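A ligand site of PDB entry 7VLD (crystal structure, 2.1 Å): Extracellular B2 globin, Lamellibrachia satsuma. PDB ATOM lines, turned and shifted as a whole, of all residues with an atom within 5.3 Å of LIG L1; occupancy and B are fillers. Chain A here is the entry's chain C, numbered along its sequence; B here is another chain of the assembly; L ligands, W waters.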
ATOM      1  N   LEU A  40      -4.554   8.174  37.536  1.00  0.00           N
ATOM      2  CA  LEU A  40      -3.830   8.095  36.275  1.00  0.00           C
ATOM      3  C   LEU A  40      -2.445   8.714  36.395  1.00  0.00           C
ATOM      4  O   LEU A  40      -1.442   8.125  35.941  1.00  0.00           O
ATOM      5  CB  LEU A  40      -4.633   8.799  35.179  1.00  0.00           C
ATOM      6  CG  LEU A  40      -3.991   8.916  33.792  1.00  0.00           C
ATOM      7  CD1 LEU A  40      -3.814   7.540  33.175  1.00  0.00           C
ATOM      8  CD2 LEU A  40      -4.816   9.814  32.885  1.00  0.00           C
ATOM      9  N   LEU A  50       0.504  16.169  29.455  1.00  0.00           N
ATOM     10  CA  LEU A  50      -0.477  16.304  28.377  1.00  0.00           C
ATOM     11  C   LEU A  50      -1.572  17.309  28.715  1.00  0.00           C
ATOM     12  O   LEU A  50      -2.303  17.734  27.821  1.00  0.00           O
ATOM     13  CB  LEU A  50      -1.106  14.937  28.073  1.00  0.00           C
ATOM     14  CG  LEU A  50      -0.116  13.813  27.755  1.00  0.00           C
ATOM     15  CD1 LEU A  50      -0.847  12.499  27.580  1.00  0.00           C
ATOM     16  CD2 LEU A  50       0.694  14.160  26.520  1.00  0.00           C
ATOM     17  N   PHE A  51      -1.695  17.689  29.987  1.00  0.00           N
ATOM     18  CA  PHE A  51      -2.756  18.564  30.457  1.00  0.00           C
ATOM     19  C   PHE A  51      -2.203  19.880  30.984  1.00  0.00           C
ATOM     20  O   PHE A  51      -2.701  20.455  31.954  1.00  0.00           O
ATOM     21  CB  PHE A  51      -3.595  17.857  31.530  1.00  0.00           C
ATOM     22  CG  PHE A  51      -4.123  16.524  31.097  1.00  0.00           C
ATOM     23  CD1 PHE A  51      -5.298  16.429  30.371  1.00  0.00           C
ATOM     24  CD2 PHE A  51      -3.437  15.357  31.419  1.00  0.00           C
ATOM     25  CE1 PHE A  51      -5.775  15.198  29.962  1.00  0.00           C
ATOM     26  CE2 PHE A  51      -3.916  14.118  31.016  1.00  0.00           C
ATOM     27  CZ  PHE A  51      -5.090  14.045  30.287  1.00  0.00           C
ATOM     28  N   ARG A  53      -2.312  22.734  29.381  1.00  0.00           N
ATOM     29  CA  ARG A  53      -3.248  23.807  29.059  1.00  0.00           C
ATOM     30  C   ARG A  53      -4.381  23.909  30.058  1.00  0.00           C
ATOM     31  O   ARG A  53      -4.980  24.985  30.188  1.00  0.00           O
ATOM     32  CB  ARG A  53      -3.800  23.602  27.648  1.00  0.00           C
ATOM     33  CG  ARG A  53      -4.403  24.859  27.034  1.00  0.00           C
ATOM     34  CD  ARG A  53      -5.324  24.524  25.869  1.00  0.00           C
ATOM     35  NE  ARG A  53      -6.538  23.854  26.331  1.00  0.00           N
ATOM     36  CZ  ARG A  53      -7.620  24.475  26.763  1.00  0.00           C
ATOM     37  NH1 ARG A  53      -8.677  23.784  27.165  1.00  0.00           N
ATOM     38  NH2 ARG A  53      -7.660  25.806  26.800  1.00  0.00           N
ATOM     39  N   VAL A  54      -4.700  22.831  30.769  1.00  0.00           N
ATOM     40  CA  VAL A  54      -5.785  22.825  31.740  1.00  0.00           C
ATOM     41  C   VAL A  54      -5.252  22.676  33.166  1.00  0.00           C
ATOM     42  O   VAL A  54      -5.993  22.261  34.051  1.00  0.00           O
ATOM     43  CB  VAL A  54      -6.823  21.735  31.408  1.00  0.00           C
ATOM     44  CG1 VAL A  54      -7.460  22.016  30.061  1.00  0.00           C
ATOM     45  CG2 VAL A  54      -6.173  20.363  31.428  1.00  0.00           C
ATOM     46  N   HIS A  67     -11.975  21.074  33.182  1.00  0.00           N
ATOM     47  CA  HIS A  67     -11.609  19.964  32.319  1.00  0.00           C
ATOM     48  C   HIS A  67     -12.221  18.660  32.816  1.00  0.00           C
ATOM     49  O   HIS A  67     -12.758  17.878  32.022  1.00  0.00           O
ATOM     50  CB  HIS A  67     -10.092  19.842  32.234  1.00  0.00           C
ATOM     51  CG  HIS A  67      -9.619  18.575  31.585  1.00  0.00           C
ATOM     52  ND1 HIS A  67      -9.727  18.350  30.233  1.00  0.00           N
ATOM     53  CD2 HIS A  67      -9.055  17.463  32.106  1.00  0.00           C
ATOM     54  CE1 HIS A  67      -9.241  17.149  29.946  1.00  0.00           C
ATOM     55  NE2 HIS A  67      -8.826  16.594  31.069  1.00  0.00           N
ATOM     56  N   ARG A  70     -15.730  18.442  31.884  1.00  0.00           N
ATOM     57  CA  ARG A  70     -15.870  18.166  30.461  1.00  0.00           C
ATOM     58  C   ARG A  70     -15.692  16.675  30.169  1.00  0.00           C
ATOM     59  O   ARG A  70     -16.474  16.079  29.425  1.00  0.00           O
ATOM     60  CB  ARG A  70     -14.874  18.988  29.642  1.00  0.00           C
ATOM     61  CG  ARG A  70     -15.262  20.443  29.446  1.00  0.00           C
ATOM     62  CD  ARG A  70     -14.449  21.121  28.357  1.00  0.00           C
ATOM     63  NE  ARG A  70     -13.033  21.246  28.709  1.00  0.00           N
ATOM     64  CZ  ARG A  70     -12.530  22.252  29.417  1.00  0.00           C
ATOM     65  NH1 ARG A  70     -13.313  23.222  29.847  1.00  0.00           N
ATOM     66  NH2 ARG A  70     -11.230  22.270  29.692  1.00  0.00           N
ATOM     67  N   VAL A  71     -14.648  16.071  30.738  1.00  0.00           N
ATOM     68  CA  VAL A  71     -14.410  14.644  30.530  1.00  0.00           C
ATOM     69  C   VAL A  71     -15.585  13.825  31.060  1.00  0.00           C
ATOM     70  O   VAL A  71     -16.077  12.907  30.395  1.00  0.00           O
ATOM     71  CB  VAL A  71     -13.086  14.216  31.197  1.00  0.00           C
ATOM     72  CG1 VAL A  71     -12.893  12.713  31.097  1.00  0.00           C
ATOM     73  CG2 VAL A  71     -11.912  14.962  30.575  1.00  0.00           C
ATOM     74  N   GLY A  74     -18.406  14.118  28.815  1.00  0.00           N
ATOM     75  CA  GLY A  74     -18.216  13.279  27.641  1.00  0.00           C
ATOM     76  C   GLY A  74     -18.510  11.818  27.921  1.00  0.00           C
ATOM     77  O   GLY A  74     -19.122  11.133  27.096  1.00  0.00           O
ATOM     78  N   LEU A  75     -18.065  11.311  29.074  1.00  0.00           N
ATOM     79  CA  LEU A  75     -18.358   9.920  29.422  1.00  0.00           C
ATOM     80  C   LEU A  75     -19.852   9.727  29.672  1.00  0.00           C
ATOM     81  O   LEU A  75     -20.417   8.701  29.277  1.00  0.00           O
ATOM     82  CB  LEU A  75     -17.544   9.499  30.649  1.00  0.00           C
ATOM     83  CG  LEU A  75     -17.689   8.018  31.014  1.00  0.00           C
ATOM     84  CD1 LEU A  75     -17.261   7.133  29.851  1.00  0.00           C
ATOM     85  CD2 LEU A  75     -16.900   7.671  32.268  1.00  0.00           C
ATOM     86  N   LEU A  95     -15.207  12.723  19.550  1.00  0.00           N
ATOM     87  CA  LEU A  95     -14.259  12.640  20.654  1.00  0.00           C
ATOM     88  C   LEU A  95     -12.886  12.166  20.171  1.00  0.00           C
ATOM     89  O   LEU A  95     -11.866  12.596  20.708  1.00  0.00           O
ATOM     90  CB  LEU A  95     -14.781  11.707  21.740  1.00  0.00           C
ATOM     91  CG  LEU A  95     -16.043  12.179  22.466  1.00  0.00           C
ATOM     92  CD1 LEU A  95     -16.591  11.097  23.373  1.00  0.00           C
ATOM     93  CD2 LEU A  95     -15.747  13.443  23.255  1.00  0.00           C
ATOM     94  N   GLN A  98     -11.013  15.080  18.756  1.00  0.00           N
ATOM     95  CA  GLN A  98     -10.614  15.977  19.831  1.00  0.00           C
ATOM     96  C   GLN A  98      -9.352  15.494  20.540  1.00  0.00           C
ATOM     97  O   GLN A  98      -8.546  16.311  20.997  1.00  0.00           O
ATOM     98  CB  GLN A  98     -11.763  16.147  20.836  1.00  0.00           C
ATOM     99  CG  GLN A  98     -12.895  17.018  20.353  1.00  0.00           C
ATOM    100  CD  GLN A  98     -13.998  17.168  21.381  1.00  0.00           C
ATOM    101  OE1 GLN A  98     -14.395  16.195  22.014  1.00  0.00           O
ATOM    102  NE2 GLN A  98     -14.491  18.384  21.559  1.00  0.00           N
ATOM    103  N   HIS A  99      -9.178  14.184  20.645  1.00  0.00           N
ATOM    104  CA  HIS A  99      -7.967  13.603  21.205  1.00  0.00           C
ATOM    105  C   HIS A  99      -6.932  13.265  20.145  1.00  0.00           C
ATOM    106  O   HIS A  99      -5.818  12.841  20.495  1.00  0.00           O
ATOM    107  CB  HIS A  99      -8.298  12.340  22.004  1.00  0.00           C
ATOM    108  CG  HIS A  99      -9.222  12.580  23.166  1.00  0.00           C
ATOM    109  ND1 HIS A  99     -10.583  12.726  23.019  1.00  0.00           N
ATOM    110  CD2 HIS A  99      -8.970  12.699  24.493  1.00  0.00           C
ATOM    111  CE1 HIS A  99     -11.130  12.925  24.198  1.00  0.00           C
ATOM    112  NE2 HIS A  99     -10.178  12.911  25.112  1.00  0.00           N
ATOM    113  N   ARG A 102      -2.743  14.774  19.411  1.00  0.00           N
ATOM    114  CA  ARG A 102      -2.036  15.414  20.521  1.00  0.00           C
ATOM    115  C   ARG A 102      -0.941  14.436  20.922  1.00  0.00           C
ATOM    116  O   ARG A 102      -1.233  13.398  21.519  1.00  0.00           O
ATOM    117  CB  ARG A 102      -2.983  15.710  21.682  1.00  0.00           C
ATOM    118  CG  ARG A 102      -4.219  16.513  21.314  1.00  0.00           C
ATOM    119  CD  ARG A 102      -5.177  16.562  22.490  1.00  0.00           C
ATOM    120  NE  ARG A 102      -6.347  17.387  22.217  1.00  0.00           N
ATOM    121  CZ  ARG A 102      -6.424  18.689  22.490  1.00  0.00           C
ATOM    122  NH1 ARG A 102      -7.532  19.370  22.210  1.00  0.00           N
ATOM    123  NH2 ARG A 102      -5.397  19.317  23.049  1.00  0.00           N
ATOM    124  N   GLY A 104       1.354  12.946  22.844  1.00  0.00           N
ATOM    125  CA  GLY A 104       1.381  11.888  23.835  1.00  0.00           C
ATOM    126  C   GLY A 104       0.059  11.233  24.167  1.00  0.00           C
ATOM    127  O   GLY A 104       0.002  10.465  25.133  1.00  0.00           O
ATOM    128  N   VAL A 105      -1.003  11.496  23.412  1.00  0.00           N
ATOM    129  CA  VAL A 105      -2.305  10.871  23.648  1.00  0.00           C
ATOM    130  C   VAL A 105      -2.373   9.608  22.787  1.00  0.00           C
ATOM    131  O   VAL A 105      -2.535   9.683  21.565  1.00  0.00           O
ATOM    132  CB  VAL A 105      -3.453  11.826  23.321  1.00  0.00           C
ATOM    133  CG1 VAL A 105      -4.787  11.144  23.533  1.00  0.00           C
ATOM    134  CG2 VAL A 105      -3.351  13.078  24.179  1.00  0.00           C
ATOM    135  N   THR A 106      -2.244   8.449  23.430  1.00  0.00           N
ATOM    136  CA  THR A 106      -2.128   7.170  22.748  1.00  0.00           C
ATOM    137  C   THR A 106      -3.172   6.196  23.286  1.00  0.00           C
ATOM    138  O   THR A 106      -3.903   6.497  24.231  1.00  0.00           O
ATOM    139  CB  THR A 106      -0.728   6.575  22.905  1.00  0.00           C
ATOM    140  OG1 THR A 106      -0.504   6.248  24.274  1.00  0.00           O
ATOM    141  CG2 THR A 106       0.337   7.569  22.442  1.00  0.00           C
ATOM    142  N   GLY A 109      -2.535   5.309  27.020  1.00  0.00           N
ATOM    143  CA  GLY A 109      -3.095   6.181  28.038  1.00  0.00           C
ATOM    144  C   GLY A 109      -4.544   5.867  28.366  1.00  0.00           C
ATOM    145  O   GLY A 109      -4.975   6.009  29.507  1.00  0.00           O
ATOM    146  N   PHE A 110      -5.303   5.423  27.362  1.00  0.00           N
ATOM    147  CA  PHE A 110      -6.699   5.047  27.600  1.00  0.00           C
ATOM    148  C   PHE A 110      -6.793   3.731  28.360  1.00  0.00           C
ATOM    149  O   PHE A 110      -7.693   3.560  29.195  1.00  0.00           O
ATOM    150  CB  PHE A 110      -7.458   4.970  26.278  1.00  0.00           C
ATOM    151  CG  PHE A 110      -7.950   6.300  25.780  1.00  0.00           C
ATOM    152  CD1 PHE A 110      -7.086   7.191  25.157  1.00  0.00           C
ATOM    153  CD2 PHE A 110      -9.276   6.665  25.936  1.00  0.00           C
ATOM    154  CE1 PHE A 110      -7.538   8.411  24.696  1.00  0.00           C
ATOM    155  CE2 PHE A 110      -9.731   7.891  25.483  1.00  0.00           C
ATOM    156  CZ  PHE A 110      -8.867   8.760  24.864  1.00  0.00           C
ATOM    157  N   ILE A 113      -6.200   4.826  31.977  1.00  0.00           N
ATOM    158  CA  ILE A 113      -7.353   5.447  32.621  1.00  0.00           C
ATOM    159  C   ILE A 113      -8.487   4.451  32.795  1.00  0.00           C
ATOM    160  O   ILE A 113      -9.333   4.636  33.685  1.00  0.00           O
ATOM    161  CB  ILE A 113      -7.811   6.692  31.826  1.00  0.00           C
ATOM    162  CG1 ILE A 113      -8.532   7.662  32.759  1.00  0.00           C
ATOM    163  CG2 ILE A 113      -8.713   6.299  30.675  1.00  0.00           C
ATOM    164  CD1 ILE A 113      -9.005   8.933  32.072  1.00  0.00           C
ATOM    165  N   PHE A 117     -10.471   4.090  36.367  1.00  0.00           N
ATOM    166  CA  PHE A 117     -11.897   3.995  36.680  1.00  0.00           C
ATOM    167  C   PHE A 117     -12.210   2.729  37.462  1.00  0.00           C
ATOM    168  O   PHE A 117     -13.007   2.746  38.399  1.00  0.00           O
ATOM    169  CB  PHE A 117     -12.715   4.038  35.384  1.00  0.00           C
ATOM    170  CG  PHE A 117     -13.045   5.428  34.913  1.00  0.00           C
ATOM    171  CD1 PHE A 117     -14.166   6.083  35.381  1.00  0.00           C
ATOM    172  CD2 PHE A 117     -12.237   6.069  33.987  1.00  0.00           C
ATOM    173  CE1 PHE A 117     -14.478   7.369  34.947  1.00  0.00           C
ATOM    174  CE2 PHE A 117     -12.535   7.336  33.547  1.00  0.00           C
ATOM    175  CZ  PHE A 117     -13.662   7.989  34.029  1.00  0.00           C
ATOM    176  N   PHE A 137     -16.984   0.107  28.819  1.00  0.00           N
ATOM    177  CA  PHE A 137     -15.983   1.172  28.841  1.00  0.00           C
ATOM    178  C   PHE A 137     -14.988   0.994  27.690  1.00  0.00           C
ATOM    179  O   PHE A 137     -14.629   1.962  27.016  1.00  0.00           O
ATOM    180  CB  PHE A 137     -15.257   1.178  30.192  1.00  0.00           C
ATOM    181  CG  PHE A 137     -14.385   2.378  30.400  1.00  0.00           C
ATOM    182  CD1 PHE A 137     -14.884   3.529  30.993  1.00  0.00           C
ATOM    183  CD2 PHE A 137     -13.049   2.359  30.027  1.00  0.00           C
ATOM    184  CE1 PHE A 137     -14.086   4.637  31.200  1.00  0.00           C
ATOM    185  CE2 PHE A 137     -12.236   3.470  30.226  1.00  0.00           C
ATOM    186  CZ  PHE A 137     -12.758   4.603  30.821  1.00  0.00           C
ATOM    187  N   ILE A 140     -16.466   1.942  24.443  1.00  0.00           N
ATOM    188  CA  ILE A 140     -16.454   3.394  24.257  1.00  0.00           C
ATOM    189  C   ILE A 140     -15.054   3.871  23.858  1.00  0.00           C
ATOM    190  O   ILE A 140     -14.893   4.632  22.905  1.00  0.00           O
ATOM    191  CB  ILE A 140     -16.957   4.100  25.528  1.00  0.00           C
ATOM    192  CG1 ILE A 140     -18.469   3.845  25.698  1.00  0.00           C
ATOM    193  CG2 ILE A 140     -16.646   5.588  25.479  1.00  0.00           C
ATOM    194  CD1 ILE A 140     -19.043   4.363  26.992  1.00  0.00           C
ATOM    195  N   THR A 141     -14.026   3.410  24.578  1.00  0.00           N
ATOM    196  CA  THR A 141     -12.672   3.869  24.282  1.00  0.00           C
ATOM    197  C   THR A 141     -12.167   3.343  22.949  1.00  0.00           C
ATOM    198  O   THR A 141     -11.314   3.984  22.316  1.00  0.00           O
ATOM    199  CB  THR A 141     -11.711   3.469  25.398  1.00  0.00           C
ATOM    200  OG1 THR A 141     -11.716   2.041  25.568  1.00  0.00           O
ATOM    201  CG2 THR A 141     -12.112   4.127  26.714  1.00  0.00           C
ATOM    202  N   MET A 144     -13.099   5.932  20.673  1.00  0.00           N
ATOM    203  CA  MET A 144     -12.379   7.177  20.925  1.00  0.00           C
ATOM    204  C   MET A 144     -10.944   7.134  20.427  1.00  0.00           C
ATOM    205  O   MET A 144     -10.347   8.191  20.201  1.00  0.00           O
ATOM    206  CB  MET A 144     -12.385   7.486  22.431  1.00  0.00           C
ATOM    207  CG  MET A 144     -13.753   7.811  23.007  1.00  0.00           C
ATOM    208  SD  MET A 144     -13.652   8.336  24.730  1.00  0.00           S
ATOM    209  CE  MET A 144     -12.652   9.818  24.582  1.00  0.00           C
ATOM    210  N   HIS B  90     -14.591  28.434  27.755  1.00  0.00           N
ATOM    211  CA  HIS B  90     -14.330  27.337  26.832  1.00  0.00           C
ATOM    212  C   HIS B  90     -15.395  27.281  25.732  1.00  0.00           C
ATOM    213  O   HIS B  90     -15.066  27.164  24.549  1.00  0.00           O
ATOM    214  CB  HIS B  90     -14.271  26.005  27.594  1.00  0.00           C
ATOM    215  CG  HIS B  90     -13.830  24.847  26.763  1.00  0.00           C
ATOM    216  ND1 HIS B  90     -12.512  24.600  26.468  1.00  0.00           N
ATOM    217  CD2 HIS B  90     -14.542  23.866  26.155  1.00  0.00           C
ATOM    218  CE1 HIS B  90     -12.419  23.521  25.725  1.00  0.00           C
ATOM    219  NE2 HIS B  90     -13.637  23.043  25.515  1.00  0.00           N
ATOM    220  N   GLN B  94     -15.129  27.835  21.607  1.00  0.00           N
ATOM    221  CA  GLN B  94     -15.718  26.864  20.695  1.00  0.00           C
ATOM    222  C   GLN B  94     -16.654  27.487  19.683  1.00  0.00           C
ATOM    223  O   GLN B  94     -17.015  26.831  18.707  1.00  0.00           O
ATOM    224  CB  GLN B  94     -16.456  25.781  21.488  1.00  0.00           C
ATOM    225  CG  GLN B  94     -15.560  24.853  22.287  1.00  0.00           C
ATOM    226  CD  GLN B  94     -16.337  23.885  23.161  1.00  0.00           C
ATOM    227  OE1 GLN B  94     -17.395  24.224  23.680  1.00  0.00           O
ATOM    228  NE2 GLN B  94     -15.823  22.670  23.306  1.00  0.00           N
HETATM  229  C1  LIG L   1      -9.836  16.690  26.393  1.00  0.00           C
HETATM  230  C2  LIG L   1     -13.119  13.182  27.125  1.00  0.00           C
HETATM  231  C3  LIG L   1      -9.574  10.043  28.219  1.00  0.00           C
HETATM  232  C4  LIG L   1      -6.299  13.373  26.850  1.00  0.00           C
HETATM  233  C5  LIG L   1     -11.036  16.031  26.526  1.00  0.00           C
HETATM  234  C6  LIG L   1     -12.363  16.614  26.400  1.00  0.00           C
HETATM  235  C7  LIG L   1     -13.265  15.642  26.593  1.00  0.00           C
HETATM  236  C8  LIG L   1     -12.544  14.407  26.864  1.00  0.00           C
HETATM  237  C9  LIG L   1     -14.797  15.800  26.561  1.00  0.00           C
HETATM  238  C10 LIG L   1     -12.710  18.088  26.084  1.00  0.00           C
HETATM  239  C11 LIG L   1     -12.424  18.414  24.625  1.00  0.00           C
HETATM  240  C12 LIG L   1     -12.930  19.804  24.303  1.00  0.00           C
HETATM  241  O1  LIG L   1     -13.890  20.260  24.964  1.00  0.00           O
HETATM  242  O2  LIG L   1     -12.367  20.444  23.388  1.00  0.00           O
HETATM  243  C13 LIG L   1     -12.451  12.026  27.512  1.00  0.00           C
HETATM  244  C14 LIG L   1     -13.073  10.779  27.904  1.00  0.00           C
HETATM  245  C15 LIG L   1     -12.083   9.905  28.215  1.00  0.00           C
HETATM  246  C16 LIG L   1     -10.819  10.587  28.012  1.00  0.00           C
HETATM  247  C17 LIG L   1     -14.608  10.583  27.949  1.00  0.00           C
HETATM  248  C18 LIG L   1     -12.178   8.435  28.690  1.00  0.00           C
HETATM  249  C19 LIG L   1     -13.296   7.708  28.738  1.00  0.00           C
HETATM  250  C20 LIG L   1      -8.369  10.660  27.932  1.00  0.00           C
HETATM  251  C21 LIG L   1      -7.042  10.081  28.082  1.00  0.00           C
HETATM  252  C22 LIG L   1      -6.133  11.000  27.702  1.00  0.00           C
HETATM  253  C23 LIG L   1      -6.862  12.188  27.303  1.00  0.00           C
HETATM  254  C24 LIG L   1      -6.804   8.642  28.591  1.00  0.00           C
HETATM  255  C25 LIG L   1      -4.589  10.918  27.652  1.00  0.00           C
HETATM  256  C26 LIG L   1      -3.862   9.840  27.977  1.00  0.00           C
HETATM  257  C27 LIG L   1      -6.964  14.568  26.651  1.00  0.00           C
HETATM  258  C28 LIG L   1      -6.342  15.844  26.357  1.00  0.00           C
HETATM  259  C29 LIG L   1      -7.305  16.760  26.230  1.00  0.00           C
HETATM  260  C30 LIG L   1      -8.583  16.098  26.438  1.00  0.00           C
HETATM  261  C31 LIG L   1      -4.818  16.097  26.208  1.00  0.00           C
HETATM  262  C32 LIG L   1      -7.085  18.255  25.916  1.00  0.00           C
HETATM  263  C33 LIG L   1      -7.426  19.071  27.160  1.00  0.00           C
HETATM  264  C34 LIG L   1      -7.450  20.544  26.806  1.00  0.00           C
HETATM  265  O3  LIG L   1      -6.355  21.122  26.620  1.00  0.00           O
HETATM  266  O4  LIG L   1      -8.556  21.111  26.726  1.00  0.00           O
HETATM  267  N1  LIG L   1     -11.195  14.688  26.815  1.00  0.00           N
HETATM  268  N2  LIG L   1     -11.080  11.877  27.585  1.00  0.00           N
HETATM  269  N3  LIG L   1      -8.212  11.950  27.452  1.00  0.00           N
HETATM  270  N4  LIG L   1      -8.322  14.767  26.694  1.00  0.00           N
HETATM  271 FE1  LIG L   1      -9.711  13.290  27.078  1.00  0.00          FE
HETATM  272  O1  LG2 L   2      -9.402  13.548  28.838  1.00  0.00           O
HETATM  273  O2  LG2 L   2      -8.722  14.213  29.588  1.00  0.00           O
HETATM  274  O   HOH W   1     -10.399  19.924  28.518  1.00  0.00           O
HETATM  275  O   HOH W   2     -17.565  17.472  27.457  1.00  0.00           O
HETATM  276  O   HOH W   3      -3.795  20.388  28.048  1.00  0.00           O
HETATM  277  O   HOH W   4     -16.234  18.984  25.740  1.00  0.00           O
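FE1 of LIG L1 is bound by NE2 of His 99 (2.1 Å). The guanidinium group (NH1) of Arg 53 is in salt-bridge range of an oxygen (O4) of LIG L1, at 2.7 Å. O1 of LIG L1 is in hydrogen-bond range of NE2 of His 90 of chain B (2.8 Å). O1 of LIG L1 lies within salt-bridge range of NE of Arg 70 (3.97 Å). O2 of LIG L1 sits close to NE2 of Gln 98. A ring nitrogen (NE2) of His 67 sits at hydrogen-bond distance from an oxygen (O2) of LG2 L2, at 2.8 Å.
An iron atom (FE1) of LIG L1 is bound by an oxygen (O1) of LG2 L2, at 1.8 Å.
A ring nitrogen (ND1) of His 99 lies within hydrogen-bond range of the backbone carbonyl oxygen of Leu 95 (2.6 Å). NE2 of His 90 of chain B lies within hydrogen-bond range of NE2 of Gln 94 of chain B, 3.1 Å away. The backbone carbonyl oxygen (O) of Gln 98 sits at hydrogen-bond distance from the guanidinium group (NE) of Arg 102 (2.7 Å). The side-chain hydroxyl (OG1) of Thr 141 lies within hydrogen-bond range of the backbone carbonyl oxygen (O) of Phe 137, 3.3 Å away.
O of Leu 50 touches C31 of LIG L1, 3.4 Å away. CE1 of Phe 51 touches C27 of LIG L1, 3.6 Å away. CG1 of Val 54 touches C34 of LIG L1, at 3.6 Å. His 67 touches LIG L1. Val 71 touches LIG L1. N of Leu 75 touches C17 of LIG L1, 3.7 Å away. Arg 102 touches LIG L1 (NH2 to C32, 3.5 Å). Val 105 touches LIG L1. O of Gly 109 touches C24 of LIG L1 (3.3 Å). CE2 of Phe 110 touches C3 of LIG L1, 3.5 Å away. CG2 of Ile 113 touches C24 of LIG L1 (3.7 Å). Phe 137 touches LIG L1 (CZ to C19, 3.8 Å). Met 144 touches LIG L1. Gln 94 of chain B touches LIG L1 (NE2 to O1, 3.5 Å). Within 4 Å of LIG L1: Leu 50, Phe 51, Arg 53, Val 54, His 67, Arg 70, Val 71, Leu 75, Gln 98, His 99, Arg 102, Val 105, Gly 109, Phe 110, Ile 113, Phe 137, Met 144, His 90 of chain B and Gln 94 of chain B.
Water W1 lies within hydrogen-bond range of a ring nitrogen (ND1) of His 67 (2.4 Å), the guanidinium group of Arg 70 (2.8 Å) and an oxygen (O4) of LIG L1 (2.8 Å). Water W3 lies within hydrogen-bond range of an oxygen (O3) of LIG L1, the backbone carbonyl oxygen of Leu 50 and the backbone NH of Arg 53.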
